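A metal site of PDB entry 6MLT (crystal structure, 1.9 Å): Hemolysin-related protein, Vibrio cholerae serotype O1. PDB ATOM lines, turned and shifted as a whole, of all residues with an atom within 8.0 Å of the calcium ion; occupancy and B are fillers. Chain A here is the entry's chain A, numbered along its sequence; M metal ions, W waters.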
ATOM      1  N   VAL A  38     -24.593 -22.914  19.082  1.00  0.00           N
ATOM      2  CA  VAL A  38     -24.903 -24.105  19.861  1.00  0.00           C
ATOM      3  C   VAL A  38     -24.363 -23.902  21.278  1.00  0.00           C
ATOM      4  O   VAL A  38     -23.492 -23.058  21.519  1.00  0.00           O
ATOM      5  CB  VAL A  38     -24.280 -25.383  19.253  1.00  0.00           C
ATOM      6  CG1 VAL A  38     -25.013 -25.797  17.984  1.00  0.00           C
ATOM      7  CG2 VAL A  38     -22.784 -25.169  18.975  1.00  0.00           C
ATOM      8  N   GLN A  39     -24.881 -24.701  22.226  1.00  0.00           N
ATOM      9  CA  GLN A  39     -24.428 -24.655  23.618  1.00  0.00           C
ATOM     10  C   GLN A  39     -23.120 -25.420  23.786  1.00  0.00           C
ATOM     11  O   GLN A  39     -23.026 -26.596  23.409  1.00  0.00           O
ATOM     12  CB  GLN A  39     -25.489 -25.259  24.534  1.00  0.00           C
ATOM     13  CG  GLN A  39     -26.870 -24.632  24.470  1.00  0.00           C
ATOM     14  CD  GLN A  39     -26.997 -23.377  25.315  1.00  0.00           C
ATOM     15  OE1 GLN A  39     -26.082 -22.998  26.038  1.00  0.00           O
ATOM     16  NE2 GLN A  39     -28.152 -22.731  25.223  1.00  0.00           N
ATOM     17  N   LEU A  40     -22.117 -24.793  24.413  1.00  0.00           N
ATOM     18  CA  LEU A  40     -20.814 -25.424  24.567  1.00  0.00           C
ATOM     19  C   LEU A  40     -20.249 -25.421  25.975  1.00  0.00           C
ATOM     20  O   LEU A  40     -19.235 -26.091  26.201  1.00  0.00           O
ATOM     21  CB  LEU A  40     -19.788 -24.757  23.636  1.00  0.00           C
ATOM     22  CG  LEU A  40     -20.053 -24.908  22.137  1.00  0.00           C
ATOM     23  CD1 LEU A  40     -19.058 -24.067  21.341  1.00  0.00           C
ATOM     24  CD2 LEU A  40     -20.002 -26.359  21.701  1.00  0.00           C
ATOM     25  N   ASN A  41     -20.847 -24.711  26.941  1.00  0.00           N
ATOM     26  CA  ASN A  41     -20.306 -24.717  28.289  1.00  0.00           C
ATOM     27  C   ASN A  41     -21.434 -24.571  29.305  1.00  0.00           C
ATOM     28  O   ASN A  41     -22.583 -24.262  28.962  1.00  0.00           O
ATOM     29  CB  ASN A  41     -19.249 -23.628  28.484  1.00  0.00           C
ATOM     30  CG  ASN A  41     -19.842 -22.235  28.573  1.00  0.00           C
ATOM     31  OD1 ASN A  41     -20.577 -21.812  27.689  1.00  0.00           O
ATOM     32  ND2 ASN A  41     -19.536 -21.522  29.652  1.00  0.00           N
ATOM     33  N   ASP A  42     -21.089 -24.805  30.571  1.00  0.00           N
ATOM     34  CA  ASP A  42     -22.049 -24.770  31.665  1.00  0.00           C
ATOM     35  C   ASP A  42     -22.034 -23.367  32.263  1.00  0.00           C
ATOM     36  O   ASP A  42     -21.233 -23.062  33.154  1.00  0.00           O
ATOM     37  CB  ASP A  42     -21.719 -25.830  32.694  1.00  0.00           C
ATOM     38  CG  ASP A  42     -22.712 -25.869  33.838  1.00  0.00           C
ATOM     39  OD1 ASP A  42     -23.801 -25.272  33.706  1.00  0.00           O
ATOM     40  OD2 ASP A  42     -22.387 -26.488  34.871  1.00  0.00           O
ATOM     41  N   ASP A  43     -22.913 -22.500  31.767  1.00  0.00           N
ATOM     42  CA  ASP A  43     -22.930 -21.109  32.232  1.00  0.00           C
ATOM     43  C   ASP A  43     -23.533 -20.979  33.626  1.00  0.00           C
ATOM     44  O   ASP A  43     -23.038 -20.195  34.441  1.00  0.00           O
ATOM     45  CB  ASP A  43     -23.700 -20.239  31.246  1.00  0.00           C
ATOM     46  CG  ASP A  43     -22.960 -20.042  29.946  1.00  0.00           C
ATOM     47  OD1 ASP A  43     -21.914 -19.369  29.957  1.00  0.00           O
ATOM     48  OD2 ASP A  43     -23.422 -20.577  28.924  1.00  0.00           O
ATOM     49  N   ASN A  44     -24.613 -21.704  33.922  1.00  0.00           N
ATOM     50  CA  ASN A  44     -25.284 -21.575  35.211  1.00  0.00           C
ATOM     51  C   ASN A  44     -24.724 -22.496  36.289  1.00  0.00           C
ATOM     52  O   ASN A  44     -25.238 -22.501  37.406  1.00  0.00           O
ATOM     53  CB  ASN A  44     -26.789 -21.820  35.059  1.00  0.00           C
ATOM     54  CG  ASN A  44     -27.121 -23.239  34.654  1.00  0.00           C
ATOM     55  OD1 ASN A  44     -26.244 -24.104  34.600  1.00  0.00           O
ATOM     56  ND2 ASN A  44     -28.389 -23.486  34.386  1.00  0.00           N
ATOM     57  N   ILE A  49     -24.907 -29.080  30.433  1.00  0.00           N
ATOM     58  CA  ILE A  49     -24.890 -28.133  29.322  1.00  0.00           C
ATOM     59  C   ILE A  49     -26.156 -28.363  28.516  1.00  0.00           C
ATOM     60  O   ILE A  49     -26.275 -29.361  27.790  1.00  0.00           O
ATOM     61  CB  ILE A  49     -23.642 -28.293  28.442  1.00  0.00           C
ATOM     62  CG1 ILE A  49     -22.383 -28.079  29.300  1.00  0.00           C
ATOM     63  CG2 ILE A  49     -23.675 -27.302  27.295  1.00  0.00           C
ATOM     64  CD1 ILE A  49     -21.084 -28.327  28.571  1.00  0.00           C
ATOM     65  N   ASP A  50     -27.117 -27.454  28.638  1.00  0.00           N
ATOM     66  CA  ASP A  50     -28.390 -27.593  27.948  1.00  0.00           C
ATOM     67  C   ASP A  50     -28.967 -26.205  27.693  1.00  0.00           C
ATOM     68  O   ASP A  50     -28.274 -25.186  27.829  1.00  0.00           O
ATOM     69  CB  ASP A  50     -29.345 -28.490  28.751  1.00  0.00           C
ATOM     70  CG  ASP A  50     -29.625 -27.964  30.133  1.00  0.00           C
ATOM     71  OD1 ASP A  50     -29.445 -26.746  30.364  1.00  0.00           O
ATOM     72  OD2 ASP A  50     -30.015 -28.766  30.999  1.00  0.00           O
ATOM     73  N   ASP A  53     -28.429 -22.874  29.579  1.00  0.00           N
ATOM     74  CA  ASP A  53     -27.195 -22.120  29.454  1.00  0.00           C
ATOM     75  C   ASP A  53     -27.316 -21.128  28.301  1.00  0.00           C
ATOM     76  O   ASP A  53     -28.344 -21.035  27.626  1.00  0.00           O
ATOM     77  CB  ASP A  53     -26.021 -23.078  29.277  1.00  0.00           C
ATOM     78  CG  ASP A  53     -25.865 -24.006  30.455  1.00  0.00           C
ATOM     79  OD1 ASP A  53     -25.621 -23.511  31.573  1.00  0.00           O
ATOM     80  OD2 ASP A  53     -26.016 -25.234  30.273  1.00  0.00           O
ATOM     81  N   VAL A  54     -26.246 -20.370  28.064  1.00  0.00           N
ATOM     82  CA  VAL A  54     -26.220 -19.342  27.028  1.00  0.00           C
ATOM     83  C   VAL A  54     -25.547 -19.913  25.799  1.00  0.00           C
ATOM     84  O   VAL A  54     -24.372 -20.305  25.855  1.00  0.00           O
ATOM     85  CB  VAL A  54     -25.517 -18.072  27.526  1.00  0.00           C
ATOM     86  CG1 VAL A  54     -25.503 -16.996  26.438  1.00  0.00           C
ATOM     87  CG2 VAL A  54     -26.187 -17.540  28.768  1.00  0.00           C
ATOM     88  N   ALA A  55     -26.263 -19.963  24.679  1.00  0.00           N
ATOM     89  CA  ALA A  55     -25.713 -20.531  23.453  1.00  0.00           C
ATOM     90  C   ALA A  55     -24.508 -19.738  22.978  1.00  0.00           C
ATOM     91  O   ALA A  55     -24.402 -18.528  23.178  1.00  0.00           O
ATOM     92  CB  ALA A  55     -26.783 -20.563  22.357  1.00  0.00           C
ATOM     93  N   ASP A  56     -23.593 -20.436  22.325  1.00  0.00           N
ATOM     94  CA  ASP A  56     -22.295 -19.912  21.948  1.00  0.00           C
ATOM     95  C   ASP A  56     -22.137 -19.900  20.430  1.00  0.00           C
ATOM     96  O   ASP A  56     -22.971 -20.426  19.698  1.00  0.00           O
ATOM     97  CB  ASP A  56     -21.210 -20.759  22.610  1.00  0.00           C
ATOM     98  CG  ASP A  56     -21.411 -20.831  24.102  1.00  0.00           C
ATOM     99  OD1 ASP A  56     -21.416 -19.738  24.722  1.00  0.00           O
ATOM    100  OD2 ASP A  56     -21.628 -21.937  24.629  1.00  0.00           O
ATOM    101  N   ILE A  57     -21.057 -19.274  19.983  1.00  0.00           N
ATOM    102  CA  ILE A  57     -20.805 -19.056  18.556  1.00  0.00           C
ATOM    103  C   ILE A  57     -19.553 -19.826  18.153  1.00  0.00           C
ATOM    104  O   ILE A  57     -18.531 -19.774  18.848  1.00  0.00           O
ATOM    105  CB  ILE A  57     -20.679 -17.554  18.237  1.00  0.00           C
ATOM    106  CG1 ILE A  57     -22.048 -16.868  18.288  1.00  0.00           C
ATOM    107  CG2 ILE A  57     -20.072 -17.349  16.844  1.00  0.00           C
ATOM    108  CD1 ILE A  57     -22.576 -16.579  19.662  1.00  0.00           C
ATOM    109  N   LEU A  76     -16.775 -19.049  20.823  1.00  0.00           N
ATOM    110  CA  LEU A  76     -16.930 -17.763  21.501  1.00  0.00           C
ATOM    111  C   LEU A  76     -18.149 -17.794  22.421  1.00  0.00           C
ATOM    112  O   LEU A  76     -19.236 -18.184  21.999  1.00  0.00           O
ATOM    113  CB  LEU A  76     -17.075 -16.631  20.489  1.00  0.00           C
ATOM    114  CG  LEU A  76     -16.012 -16.581  19.404  1.00  0.00           C
ATOM    115  CD1 LEU A  76     -16.257 -15.413  18.459  1.00  0.00           C
ATOM    116  CD2 LEU A  76     -14.619 -16.503  20.035  1.00  0.00           C
ATOM    117  N   SER A  77     -17.960 -17.342  23.653  1.00  0.00           N
ATOM    118  CA  SER A  77     -19.050 -17.357  24.627  1.00  0.00           C
ATOM    119  C   SER A  77     -20.182 -16.431  24.186  1.00  0.00           C
ATOM    120  O   SER A  77     -19.954 -15.269  23.826  1.00  0.00           O
ATOM    121  CB  SER A  77     -18.533 -16.905  25.995  1.00  0.00           C
ATOM    122  OG  SER A  77     -19.611 -16.821  26.913  1.00  0.00           O
ATOM    123  N   GLY A  78     -21.412 -16.935  24.237  1.00  0.00           N
ATOM    124  CA  GLY A  78     -22.559 -16.099  23.937  1.00  0.00           C
ATOM    125  C   GLY A  78     -22.712 -14.926  24.885  1.00  0.00           C
ATOM    126  O   GLY A  78     -23.333 -13.917  24.522  1.00  0.00           O
ATOM    127  N   VAL A  79     -22.151 -15.031  26.092  1.00  0.00           N
ATOM    128  CA  VAL A  79     -22.287 -13.971  27.088  1.00  0.00           C
ATOM    129  C   VAL A  79     -21.483 -12.743  26.681  1.00  0.00           C
ATOM    130  O   VAL A  79     -22.015 -11.624  26.648  1.00  0.00           O
ATOM    131  CB  VAL A  79     -21.839 -14.493  28.472  1.00  0.00           C
ATOM    132  CG1 VAL A  79     -21.844 -13.364  29.521  1.00  0.00           C
ATOM    133  CG2 VAL A  79     -22.725 -15.632  28.925  1.00  0.00           C
ATOM    134  N   LEU A  84     -13.896 -19.818  24.628  1.00  0.00           N
ATOM    135  CA  LEU A  84     -14.196 -20.883  25.569  1.00  0.00           C
ATOM    136  C   LEU A  84     -13.126 -21.970  25.607  1.00  0.00           C
ATOM    137  O   LEU A  84     -13.055 -22.703  26.597  1.00  0.00           O
ATOM    138  CB  LEU A  84     -15.536 -21.533  25.214  1.00  0.00           C
ATOM    139  CG  LEU A  84     -16.763 -20.641  25.342  1.00  0.00           C
ATOM    140  CD1 LEU A  84     -17.976 -21.323  24.751  1.00  0.00           C
ATOM    141  CD2 LEU A  84     -17.010 -20.303  26.808  1.00  0.00           C
ATOM    142  N   LEU A 529     -29.740 -16.326  22.409  1.00  0.00           N
ATOM    143  CA  LEU A 529     -28.673 -17.054  23.092  1.00  0.00           C
ATOM    144  C   LEU A 529     -29.078 -17.412  24.525  1.00  0.00           C
ATOM    145  O   LEU A 529     -28.850 -18.536  24.970  1.00  0.00           O
ATOM    146  CB  LEU A 529     -27.397 -16.224  23.085  1.00  0.00           C
ATOM    147  CG  LEU A 529     -26.913 -15.742  21.703  1.00  0.00           C
ATOM    148  CD1 LEU A 529     -25.642 -14.906  21.831  1.00  0.00           C
ATOM    149  CD2 LEU A 529     -26.696 -16.899  20.748  1.00  0.00           C
HETATM  150 CA    CA M   1     -22.364 -20.791  26.708  1.00  0.00          CA
HETATM  151  O   HOH W   1     -21.511 -18.745  27.492  1.00  0.00           O
HETATM  152  O   HOH W   2     -23.442 -23.075  26.880  1.00  0.00           O
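Water W1 lies within hydrogen-bond range of OD1 of Asp 43 and OG of Ser 77. Water W2 lies within hydrogen-bond range of O of Asn 41, OE1 of Gln 39 and N of Leu 40.
The calcium ion is bound by the backbone carbonyl oxygen (O) of Val 54. The calcium ion is bound by the side-chain amide oxygen (OD1) of Asn 41, at 2.3 Å. The calcium ion is bound by water W1 (2.4 Å). The calcium ion is bound by OD1 of Asp 56 (2.4 Å). OD2 of Asp 43 binds the calcium ion (2.5 Å). The side-chain carboxylate (OD2) of Asp 56 binds the calcium ion, at 2.5 Å. The calcium ion is bound by water W2 (2.5 Å). The calcium ion has seven donor atoms within binding distance.
The backbone NH (N) of Val 54 lies close to the side-chain amide oxygen (OE1) of Gln 39, 3.3 Å away. The side-chain carboxylate (OD2) of Asp 56 lies close to the backbone NH (N) of Leu 40, at 2.9 Å. OD1 of Asp 56 lies close to N of Gly 78. N of Asp 56 lies within hydrogen-bond range of O of Val 38, at 2.7 Å. The side-chain carboxylate (OD1) of Asp 53 lies close to the backbone NH (N) of Asp 43.
Within 4 Å of the calcium ion: Asn 41, Asp 43, Val 54 and Asp 56. The nearest printed residue that does not touch the calcium ion is Gln 39 (4.4 Å).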
